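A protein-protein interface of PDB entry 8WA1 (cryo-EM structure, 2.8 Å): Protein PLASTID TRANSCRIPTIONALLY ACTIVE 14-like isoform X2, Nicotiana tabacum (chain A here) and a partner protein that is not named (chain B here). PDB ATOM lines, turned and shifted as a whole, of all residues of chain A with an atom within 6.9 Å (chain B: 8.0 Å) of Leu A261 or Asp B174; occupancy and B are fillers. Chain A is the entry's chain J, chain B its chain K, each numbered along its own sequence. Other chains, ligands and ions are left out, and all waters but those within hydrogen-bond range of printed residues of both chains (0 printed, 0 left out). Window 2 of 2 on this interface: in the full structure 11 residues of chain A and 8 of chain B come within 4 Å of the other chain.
The side-chain hydroxyl (OH) of Tyr B176 sits at hydrogen-bond distance from the side-chain carboxylate (OD1) of Asp B174, at 2.8 Å.
OE1 of Glu B135 sits at hydrogen-bond distance from OH of Tyr B176 (2.9 Å).
The guanidinium group (NE) of Arg B132 is in salt-bridge range of the side-chain carboxylate (OD2) of Asp B174.
NH1 of Arg B132 touches O of Ala A258 (3.9 Å).
Glu B135 touches Leu A261.
Leu A261 touches Asp B174.
NH2 of Arg A265 lies within salt-bridge range of OD2 of Asp B172 (3.5 Å).
O of Val A259 lies within hydrogen-bond range of NH2 of Arg B132 (3.1 Å).
Of the 20 printed residues of chain B, 4 touch a printed residue of chain A.
Along chain B the printed residues that touch a printed residue of chain A span positions 132 to 174.
Of the 10 printed residues of chain A, 4 touch a printed residue of chain B.
Hydrophobic or aromatic side chains of chain A within 4 Å of the printed part of chain B: Leu A261.
Among the printed residues, 5 pairs touch across the chains.
Of chain B, only Glu B135 (3.4 Å) and Asp B174 (3.4 Å) come within 4 Å of Leu A261.
Asp B174 touches just one residue of chain A: Leu A261 (3.4 Å).
Printed residues of chain A within 4 Å of Glu B135: Leu A261 (3.4 Å).
Of the printed residues of chain B, Val A259 touches Arg B132 (3.1 Å).
The nearest residue of chain A that does not touch Asp B174 is Pro A260 (4.7 Å).
The nearest printed residue of chain B that does not touch Arg A265 is Lys B140 (4.5 Å).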
ATOM      1  N   ALA A 258     -21.402   0.239  20.257  1.00  0.00           N
ATOM      2  CA  ALA A 258     -20.891  -0.916  19.527  1.00  0.00           C
ATOM      3  C   ALA A 258     -19.491  -0.699  18.967  1.00  0.00           C
ATOM      4  O   ALA A 258     -18.937  -1.623  18.362  1.00  0.00           O
ATOM      5  CB  ALA A 258     -21.848  -1.281  18.391  1.00  0.00           C
ATOM      6  N   VAL A 259     -18.913   0.485  19.147  1.00  0.00           N
ATOM      7  CA  VAL A 259     -17.586   0.802  18.621  1.00  0.00           C
ATOM      8  C   VAL A 259     -16.555  -0.065  19.339  1.00  0.00           C
ATOM      9  O   VAL A 259     -16.768  -0.445  20.501  1.00  0.00           O
ATOM     10  CB  VAL A 259     -17.286   2.305  18.768  1.00  0.00           C
ATOM     11  CG1 VAL A 259     -16.437   2.589  20.001  1.00  0.00           C
ATOM     12  CG2 VAL A 259     -16.634   2.856  17.506  1.00  0.00           C
ATOM     13  N   PRO A 260     -15.451  -0.436  18.686  1.00  0.00           N
ATOM     14  CA  PRO A 260     -14.432  -1.248  19.364  1.00  0.00           C
ATOM     15  C   PRO A 260     -13.802  -0.510  20.536  1.00  0.00           C
ATOM     16  O   PRO A 260     -13.903   0.712  20.661  1.00  0.00           O
ATOM     17  CB  PRO A 260     -13.404  -1.521  18.260  1.00  0.00           C
ATOM     18  CG  PRO A 260     -14.173  -1.394  16.991  1.00  0.00           C
ATOM     19  CD  PRO A 260     -15.184  -0.314  17.242  1.00  0.00           C
ATOM     20  N   LEU A 261     -13.138  -1.281  21.402  1.00  0.00           N
ATOM     21  CA  LEU A 261     -12.549  -0.708  22.609  1.00  0.00           C
ATOM     22  C   LEU A 261     -11.397   0.234  22.275  1.00  0.00           C
ATOM     23  O   LEU A 261     -11.168   1.221  22.986  1.00  0.00           O
ATOM     24  CB  LEU A 261     -12.079  -1.825  23.540  1.00  0.00           C
ATOM     25  CG  LEU A 261     -11.427  -1.397  24.857  1.00  0.00           C
ATOM     26  CD1 LEU A 261     -12.396  -0.582  25.701  1.00  0.00           C
ATOM     27  CD2 LEU A 261     -10.931  -2.608  25.625  1.00  0.00           C
ATOM     28  N   LYS A 262     -10.658  -0.053  21.201  1.00  0.00           N
ATOM     29  CA  LYS A 262      -9.541   0.807  20.821  1.00  0.00           C
ATOM     30  C   LYS A 262     -10.021   2.199  20.426  1.00  0.00           C
ATOM     31  O   LYS A 262      -9.305   3.188  20.620  1.00  0.00           O
ATOM     32  CB  LYS A 262      -8.742   0.163  19.690  1.00  0.00           C
ATOM     33  CG  LYS A 262      -9.589  -0.437  18.584  1.00  0.00           C
ATOM     34  CD  LYS A 262      -8.734  -1.237  17.615  1.00  0.00           C
ATOM     35  CE  LYS A 262      -9.578  -1.896  16.537  1.00  0.00           C
ATOM     36  NZ  LYS A 262      -8.748  -2.710  15.608  1.00  0.00           N
ATOM     37  N   ILE A 263     -11.229   2.297  19.866  1.00  0.00           N
ATOM     38  CA  ILE A 263     -11.801   3.607  19.572  1.00  0.00           C
ATOM     39  C   ILE A 263     -12.390   4.227  20.833  1.00  0.00           C
ATOM     40  O   ILE A 263     -12.243   5.431  21.077  1.00  0.00           O
ATOM     41  CB  ILE A 263     -12.859   3.494  18.459  1.00  0.00           C
ATOM     42  CG1 ILE A 263     -12.205   3.147  17.124  1.00  0.00           C
ATOM     43  CG2 ILE A 263     -13.647   4.789  18.336  1.00  0.00           C
ATOM     44  CD1 ILE A 263     -13.179   3.155  15.971  1.00  0.00           C
ATOM     45  N   LYS A 264     -13.063   3.417  21.654  1.00  0.00           N
ATOM     46  CA  LYS A 264     -13.746   3.949  22.829  1.00  0.00           C
ATOM     47  C   LYS A 264     -12.758   4.536  23.829  1.00  0.00           C
ATOM     48  O   LYS A 264     -13.057   5.536  24.492  1.00  0.00           O
ATOM     49  CB  LYS A 264     -14.587   2.851  23.484  1.00  0.00           C
ATOM     50  CG  LYS A 264     -15.444   3.331  24.641  1.00  0.00           C
ATOM     51  CD  LYS A 264     -16.326   2.213  25.168  1.00  0.00           C
ATOM     52  CE  LYS A 264     -17.223   1.659  24.074  1.00  0.00           C
ATOM     53  NZ  LYS A 264     -18.113   2.706  23.500  1.00  0.00           N
ATOM     54  N   ARG A 265     -11.574   3.932  23.949  1.00  0.00           N
ATOM     55  CA  ARG A 265     -10.584   4.442  24.891  1.00  0.00           C
ATOM     56  C   ARG A 265     -10.022   5.787  24.449  1.00  0.00           C
ATOM     57  O   ARG A 265      -9.442   6.513  25.265  1.00  0.00           O
ATOM     58  CB  ARG A 265      -9.455   3.427  25.074  1.00  0.00           C
ATOM     59  CG  ARG A 265      -8.666   3.128  23.814  1.00  0.00           C
ATOM     60  CD  ARG A 265      -7.671   2.006  24.053  1.00  0.00           C
ATOM     61  NE  ARG A 265      -6.918   1.675  22.848  1.00  0.00           N
ATOM     62  CZ  ARG A 265      -6.046   0.677  22.764  1.00  0.00           C
ATOM     63  NH1 ARG A 265      -5.814  -0.095  23.817  1.00  0.00           N
ATOM     64  NH2 ARG A 265      -5.406   0.447  21.625  1.00  0.00           N
ATOM     65  N   LEU A 266     -10.176   6.138  23.168  1.00  0.00           N
ATOM     66  CA  LEU A 266      -9.692   7.433  22.697  1.00  0.00           C
ATOM     67  C   LEU A 266     -10.445   8.577  23.366  1.00  0.00           C
ATOM     68  O   LEU A 266      -9.843   9.403  24.062  1.00  0.00           O
ATOM     69  CB  LEU A 266      -9.821   7.529  21.176  1.00  0.00           C
ATOM     70  CG  LEU A 266      -9.148   6.452  20.321  1.00  0.00           C
ATOM     71  CD1 LEU A 266      -9.366   6.732  18.841  1.00  0.00           C
ATOM     72  CD2 LEU A 266      -7.667   6.357  20.632  1.00  0.00           C
ATOM     73  N   ARG A 268     -13.596   8.583  25.727  1.00  0.00           N
ATOM     74  CA  ARG A 268     -14.663   7.927  26.475  1.00  0.00           C
ATOM     75  C   ARG A 268     -15.790   8.903  26.790  1.00  0.00           C
ATOM     76  O   ARG A 268     -16.969   8.530  26.773  1.00  0.00           O
ATOM     77  CB  ARG A 268     -14.104   7.319  27.761  1.00  0.00           C
ATOM     78  CG  ARG A 268     -12.793   6.573  27.572  1.00  0.00           C
ATOM     79  CD  ARG A 268     -12.349   5.889  28.854  1.00  0.00           C
ATOM     80  NE  ARG A 268     -13.196   4.748  29.186  1.00  0.00           N
ATOM     81  CZ  ARG A 268     -12.971   3.507  28.769  1.00  0.00           C
ATOM     82  NH1 ARG A 268     -11.922   3.244  28.001  1.00  0.00           N
ATOM     83  NH2 ARG A 268     -13.793   2.527  29.117  1.00  0.00           N
ATOM     84  N   VAL B 129     -16.819 -15.902  24.105  1.00  0.00           N
ATOM     85  CA  VAL B 129     -17.834 -15.723  25.140  1.00  0.00           C
ATOM     86  C   VAL B 129     -19.021 -14.935  24.598  1.00  0.00           C
ATOM     87  O   VAL B 129     -20.148 -15.072  25.087  1.00  0.00           O
ATOM     88  CB  VAL B 129     -17.218 -15.046  26.379  1.00  0.00           C
ATOM     89  CG1 VAL B 129     -16.155 -15.940  26.990  1.00  0.00           C
ATOM     90  CG2 VAL B 129     -16.634 -13.690  26.014  1.00  0.00           C
ATOM     91  N   ASP B 130     -18.784 -14.096  23.589  1.00  0.00           N
ATOM     92  CA  ASP B 130     -19.748 -13.252  22.879  1.00  0.00           C
ATOM     93  C   ASP B 130     -20.216 -12.054  23.703  1.00  0.00           C
ATOM     94  O   ASP B 130     -21.083 -11.310  23.227  1.00  0.00           O
ATOM     95  CB  ASP B 130     -20.987 -14.027  22.399  1.00  0.00           C
ATOM     96  CG  ASP B 130     -20.644 -15.097  21.385  1.00  0.00           C
ATOM     97  OD1 ASP B 130     -19.458 -15.207  21.013  1.00  0.00           O
ATOM     98  OD2 ASP B 130     -21.562 -15.830  20.960  1.00  0.00           O
ATOM     99  N   TYR B 131     -19.688 -11.837  24.904  1.00  0.00           N
ATOM    100  CA  TYR B 131     -19.990 -10.647  25.691  1.00  0.00           C
ATOM    101  C   TYR B 131     -18.692  -9.929  26.032  1.00  0.00           C
ATOM    102  O   TYR B 131     -17.727 -10.560  26.476  1.00  0.00           O
ATOM    103  CB  TYR B 131     -20.768 -10.994  26.968  1.00  0.00           C
ATOM    104  CG  TYR B 131     -20.174 -12.112  27.798  1.00  0.00           C
ATOM    105  CD1 TYR B 131     -19.199 -11.855  28.754  1.00  0.00           C
ATOM    106  CD2 TYR B 131     -20.606 -13.421  27.641  1.00  0.00           C
ATOM    107  CE1 TYR B 131     -18.660 -12.873  29.514  1.00  0.00           C
ATOM    108  CE2 TYR B 131     -20.075 -14.446  28.399  1.00  0.00           C
ATOM    109  CZ  TYR B 131     -19.101 -14.167  29.334  1.00  0.00           C
ATOM    110  OH  TYR B 131     -18.569 -15.185  30.091  1.00  0.00           O
ATOM    111  N   ARG B 132     -18.673  -8.626  25.833  1.00  0.00           N
ATOM    112  CA  ARG B 132     -17.495  -7.872  26.123  1.00  0.00           C
ATOM    113  C   ARG B 132     -17.365  -7.537  27.589  1.00  0.00           C
ATOM    114  O   ARG B 132     -18.163  -6.782  28.105  1.00  0.00           O
ATOM    115  CB  ARG B 132     -17.501  -6.637  25.263  1.00  0.00           C
ATOM    116  CG  ARG B 132     -16.975  -6.876  23.863  1.00  0.00           C
ATOM    117  CD  ARG B 132     -17.595  -5.915  22.867  1.00  0.00           C
ATOM    118  NE  ARG B 132     -17.488  -4.527  23.302  1.00  0.00           N
ATOM    119  CZ  ARG B 132     -17.351  -3.495  22.477  1.00  0.00           C
ATOM    120  NH1 ARG B 132     -17.294  -3.692  21.168  1.00  0.00           N
ATOM    121  NH2 ARG B 132     -17.263  -2.266  22.960  1.00  0.00           N
ATOM    122  N   ILE B 133     -16.359  -8.058  28.267  1.00  0.00           N
ATOM    123  CA  ILE B 133     -16.159  -7.864  29.699  1.00  0.00           C
ATOM    124  C   ILE B 133     -15.562  -6.485  29.934  1.00  0.00           C
ATOM    125  O   ILE B 133     -15.065  -5.843  29.002  1.00  0.00           O
ATOM    126  CB  ILE B 133     -15.257  -8.961  30.293  1.00  0.00           C
ATOM    127  CG1 ILE B 133     -13.834  -8.827  29.753  1.00  0.00           C
ATOM    128  CG2 ILE B 133     -15.818 -10.339  29.981  1.00  0.00           C
ATOM    129  CD1 ILE B 133     -12.860  -9.819  30.342  1.00  0.00           C
ATOM    130  N   ASN B 134     -15.604  -6.023  31.179  1.00  0.00           N
ATOM    131  CA  ASN B 134     -15.002  -4.756  31.569  1.00  0.00           C
ATOM    132  C   ASN B 134     -13.577  -5.023  32.033  1.00  0.00           C
ATOM    133  O   ASN B 134     -13.368  -5.581  33.116  1.00  0.00           O
ATOM    134  CB  ASN B 134     -15.815  -4.079  32.672  1.00  0.00           C
ATOM    135  CG  ASN B 134     -15.228  -2.747  33.096  1.00  0.00           C
ATOM    136  OD1 ASN B 134     -14.511  -2.099  32.333  1.00  0.00           O
ATOM    137  ND2 ASN B 134     -15.531  -2.332  34.320  1.00  0.00           N
ATOM    138  N   GLU B 135     -12.603  -4.614  31.224  1.00  0.00           N
ATOM    139  CA  GLU B 135     -11.196  -4.886  31.495  1.00  0.00           C
ATOM    140  C   GLU B 135     -10.652  -4.104  32.682  1.00  0.00           C
ATOM    141  O   GLU B 135      -9.505  -4.330  33.082  1.00  0.00           O
ATOM    142  CB  GLU B 135     -10.352  -4.584  30.252  1.00  0.00           C
ATOM    143  CG  GLU B 135     -10.699  -5.430  29.042  1.00  0.00           C
ATOM    144  CD  GLU B 135      -9.842  -5.100  27.837  1.00  0.00           C
ATOM    145  OE1 GLU B 135     -10.070  -5.695  26.764  1.00  0.00           O
ATOM    146  OE2 GLU B 135      -8.941  -4.244  27.966  1.00  0.00           O
ATOM    147  N   GLU B 136     -11.444  -3.196  33.258  1.00  0.00           N
ATOM    148  CA  GLU B 136     -11.003  -2.483  34.451  1.00  0.00           C
ATOM    149  C   GLU B 136     -10.920  -3.412  35.655  1.00  0.00           C
ATOM    150  O   GLU B 136     -10.104  -3.191  36.557  1.00  0.00           O
ATOM    151  CB  GLU B 136     -11.944  -1.308  34.730  1.00  0.00           C
ATOM    152  CG  GLU B 136     -11.564  -0.452  35.930  1.00  0.00           C
ATOM    153  CD  GLU B 136     -12.297  -0.860  37.194  1.00  0.00           C
ATOM    154  OE1 GLU B 136     -13.289  -1.612  37.088  1.00  0.00           O
ATOM    155  OE2 GLU B 136     -11.884  -0.428  38.289  1.00  0.00           O
ATOM    156  N   LYS B 140      -4.589  -7.317  32.908  1.00  0.00           N
ATOM    157  CA  LYS B 140      -4.243  -7.388  31.495  1.00  0.00           C
ATOM    158  C   LYS B 140      -2.760  -7.702  31.371  1.00  0.00           C
ATOM    159  O   LYS B 140      -1.913  -6.868  31.714  1.00  0.00           O
ATOM    160  CB  LYS B 140      -4.581  -6.084  30.772  1.00  0.00           C
ATOM    161  CG  LYS B 140      -4.334  -6.141  29.273  1.00  0.00           C
ATOM    162  CD  LYS B 140      -4.725  -4.843  28.587  1.00  0.00           C
ATOM    163  CE  LYS B 140      -4.513  -4.933  27.084  1.00  0.00           C
ATOM    164  NZ  LYS B 140      -4.888  -3.669  26.394  1.00  0.00           N
ATOM    165  N   PHE B 149      -6.175 -12.185  30.370  1.00  0.00           N
ATOM    166  CA  PHE B 149      -6.964 -11.436  31.338  1.00  0.00           C
ATOM    167  C   PHE B 149      -7.290 -12.324  32.529  1.00  0.00           C
ATOM    168  O   PHE B 149      -7.755 -13.455  32.357  1.00  0.00           O
ATOM    169  CB  PHE B 149      -8.253 -10.904  30.705  1.00  0.00           C
ATOM    170  CG  PHE B 149      -8.020  -9.913  29.603  1.00  0.00           C
ATOM    171  CD1 PHE B 149      -7.882 -10.335  28.291  1.00  0.00           C
ATOM    172  CD2 PHE B 149      -7.938  -8.558  29.879  1.00  0.00           C
ATOM    173  CE1 PHE B 149      -7.666  -9.423  27.276  1.00  0.00           C
ATOM    174  CE2 PHE B 149      -7.723  -7.643  28.867  1.00  0.00           C
ATOM    175  CZ  PHE B 149      -7.588  -8.077  27.564  1.00  0.00           C
ATOM    176  N   VAL B 168      -8.474 -15.101  26.950  1.00  0.00           N
ATOM    177  CA  VAL B 168      -7.342 -14.852  26.064  1.00  0.00           C
ATOM    178  C   VAL B 168      -7.863 -14.183  24.800  1.00  0.00           C
ATOM    179  O   VAL B 168      -8.914 -14.565  24.272  1.00  0.00           O
ATOM    180  CB  VAL B 168      -6.575 -16.152  25.734  1.00  0.00           C
ATOM    181  CG1 VAL B 168      -7.508 -17.201  25.145  1.00  0.00           C
ATOM    182  CG2 VAL B 168      -5.412 -15.868  24.792  1.00  0.00           C
ATOM    183  N   THR B 169      -7.143 -13.175  24.328  1.00  0.00           N
ATOM    184  CA  THR B 169      -7.539 -12.385  23.175  1.00  0.00           C
ATOM    185  C   THR B 169      -6.381 -12.263  22.200  1.00  0.00           C
ATOM    186  O   THR B 169      -5.212 -12.360  22.593  1.00  0.00           O
ATOM    187  CB  THR B 169      -8.000 -10.981  23.594  1.00  0.00           C
ATOM    188  OG1 THR B 169      -6.949 -10.326  24.315  1.00  0.00           O
ATOM    189  CG2 THR B 169      -9.235 -11.060  24.471  1.00  0.00           C
ATOM    190  N   PRO B 170      -6.671 -12.057  20.918  1.00  0.00           N
ATOM    191  CA  PRO B 170      -5.613 -11.736  19.954  1.00  0.00           C
ATOM    192  C   PRO B 170      -4.952 -10.416  20.306  1.00  0.00           C
ATOM    193  O   PRO B 170      -5.498  -9.639  21.104  1.00  0.00           O
ATOM    194  CB  PRO B 170      -6.370 -11.650  18.618  1.00  0.00           C
ATOM    195  CG  PRO B 170      -7.600 -12.464  18.828  1.00  0.00           C
ATOM    196  CD  PRO B 170      -7.975 -12.252  20.262  1.00  0.00           C
ATOM    197  N   PRO B 171      -3.778 -10.124  19.744  1.00  0.00           N
ATOM    198  CA  PRO B 171      -3.071  -8.892  20.120  1.00  0.00           C
ATOM    199  C   PRO B 171      -3.884  -7.649  19.786  1.00  0.00           C
ATOM    200  O   PRO B 171      -4.189  -7.377  18.622  1.00  0.00           O
ATOM    201  CB  PRO B 171      -1.775  -8.961  19.303  1.00  0.00           C
ATOM    202  CG  PRO B 171      -2.083  -9.889  18.175  1.00  0.00           C
ATOM    203  CD  PRO B 171      -3.027 -10.900  18.742  1.00  0.00           C
ATOM    204  N   ASP B 172      -4.227  -6.893  20.829  1.00  0.00           N
ATOM    205  CA  ASP B 172      -5.012  -5.664  20.710  1.00  0.00           C
ATOM    206  C   ASP B 172      -6.335  -5.921  19.988  1.00  0.00           C
ATOM    207  O   ASP B 172      -6.674  -5.268  19.000  1.00  0.00           O
ATOM    208  CB  ASP B 172      -4.208  -4.564  20.014  1.00  0.00           C
ATOM    209  CG  ASP B 172      -4.790  -3.182  20.245  1.00  0.00           C
ATOM    210  OD1 ASP B 172      -5.731  -3.060  21.058  1.00  0.00           O
ATOM    211  OD2 ASP B 172      -4.307  -2.218  19.615  1.00  0.00           O
ATOM    212  N   THR B 173      -7.082  -6.898  20.493  1.00  0.00           N
ATOM    213  CA  THR B 173      -8.387  -7.245  19.951  1.00  0.00           C
ATOM    214  C   THR B 173      -9.380  -7.387  21.096  1.00  0.00           C
ATOM    215  O   THR B 173      -9.028  -7.802  22.203  1.00  0.00           O
ATOM    216  CB  THR B 173      -8.328  -8.543  19.129  1.00  0.00           C
ATOM    217  OG1 THR B 173      -7.186  -8.509  18.265  1.00  0.00           O
ATOM    218  CG2 THR B 173      -9.583  -8.703  18.279  1.00  0.00           C
ATOM    219  N   ASP B 174     -10.635  -7.041  20.814  1.00  0.00           N
ATOM    220  CA  ASP B 174     -11.701  -7.078  21.805  1.00  0.00           C
ATOM    221  C   ASP B 174     -12.549  -8.340  21.702  1.00  0.00           C
ATOM    222  O   ASP B 174     -13.622  -8.408  22.311  1.00  0.00           O
ATOM    223  CB  ASP B 174     -12.583  -5.833  21.668  1.00  0.00           C
ATOM    224  CG  ASP B 174     -13.304  -5.483  22.954  1.00  0.00           C
ATOM    225  OD1 ASP B 174     -13.052  -6.152  23.975  1.00  0.00           O
ATOM    226  OD2 ASP B 174     -14.118  -4.537  22.945  1.00  0.00           O
ATOM    227  N   ILE B 175     -12.097  -9.336  20.945  1.00  0.00           N
ATOM    228  CA  ILE B 175     -12.814 -10.598  20.791  1.00  0.00           C
ATOM    229  C   ILE B 175     -12.259 -11.562  21.834  1.00  0.00           C
ATOM    230  O   ILE B 175     -11.179 -12.130  21.663  1.00  0.00           O
ATOM    231  CB  ILE B 175     -12.682 -11.157  19.374  1.00  0.00           C
ATOM    232  CG1 ILE B 175     -13.215 -10.152  18.351  1.00  0.00           C
ATOM    233  CG2 ILE B 175     -13.418 -12.483  19.254  1.00  0.00           C
ATOM    234  CD1 ILE B 175     -13.108 -10.626  16.918  1.00  0.00           C
ATOM    235  N   TYR B 176     -13.001 -11.745  22.923  1.00  0.00           N
ATOM    236  CA  TYR B 176     -12.548 -12.591  24.014  1.00  0.00           C
ATOM    237  C   TYR B 176     -12.770 -14.066  23.688  1.00  0.00           C
ATOM    238  O   TYR B 176     -13.581 -14.430  22.833  1.00  0.00           O
ATOM    239  CB  TYR B 176     -13.271 -12.225  25.311  1.00  0.00           C
ATOM    240  CG  TYR B 176     -13.134 -10.768  25.684  1.00  0.00           C
ATOM    241  CD1 TYR B 176     -12.059 -10.322  26.441  1.00  0.00           C
ATOM    242  CD2 TYR B 176     -14.076  -9.836  25.273  1.00  0.00           C
ATOM    243  CE1 TYR B 176     -11.927  -8.990  26.779  1.00  0.00           C
ATOM    244  CE2 TYR B 176     -13.955  -8.505  25.609  1.00  0.00           C
ATOM    245  CZ  TYR B 176     -12.879  -8.085  26.361  1.00  0.00           C
ATOM    246  OH  TYR B 176     -12.755  -6.756  26.696  1.00  0.00           O
ATOM    247  N   ALA B 177     -12.027 -14.918  24.388  1.00  0.00           N
ATOM    248  CA  ALA B 177     -12.124 -16.359  24.207  1.00  0.00           C
ATOM    249  C   ALA B 177     -11.715 -17.034  25.508  1.00  0.00           C
ATOM    250  O   ALA B 177     -11.249 -16.383  26.447  1.00  0.00           O
ATOM    251  CB  ALA B 177     -11.258 -16.837  23.038  1.00  0.00           C
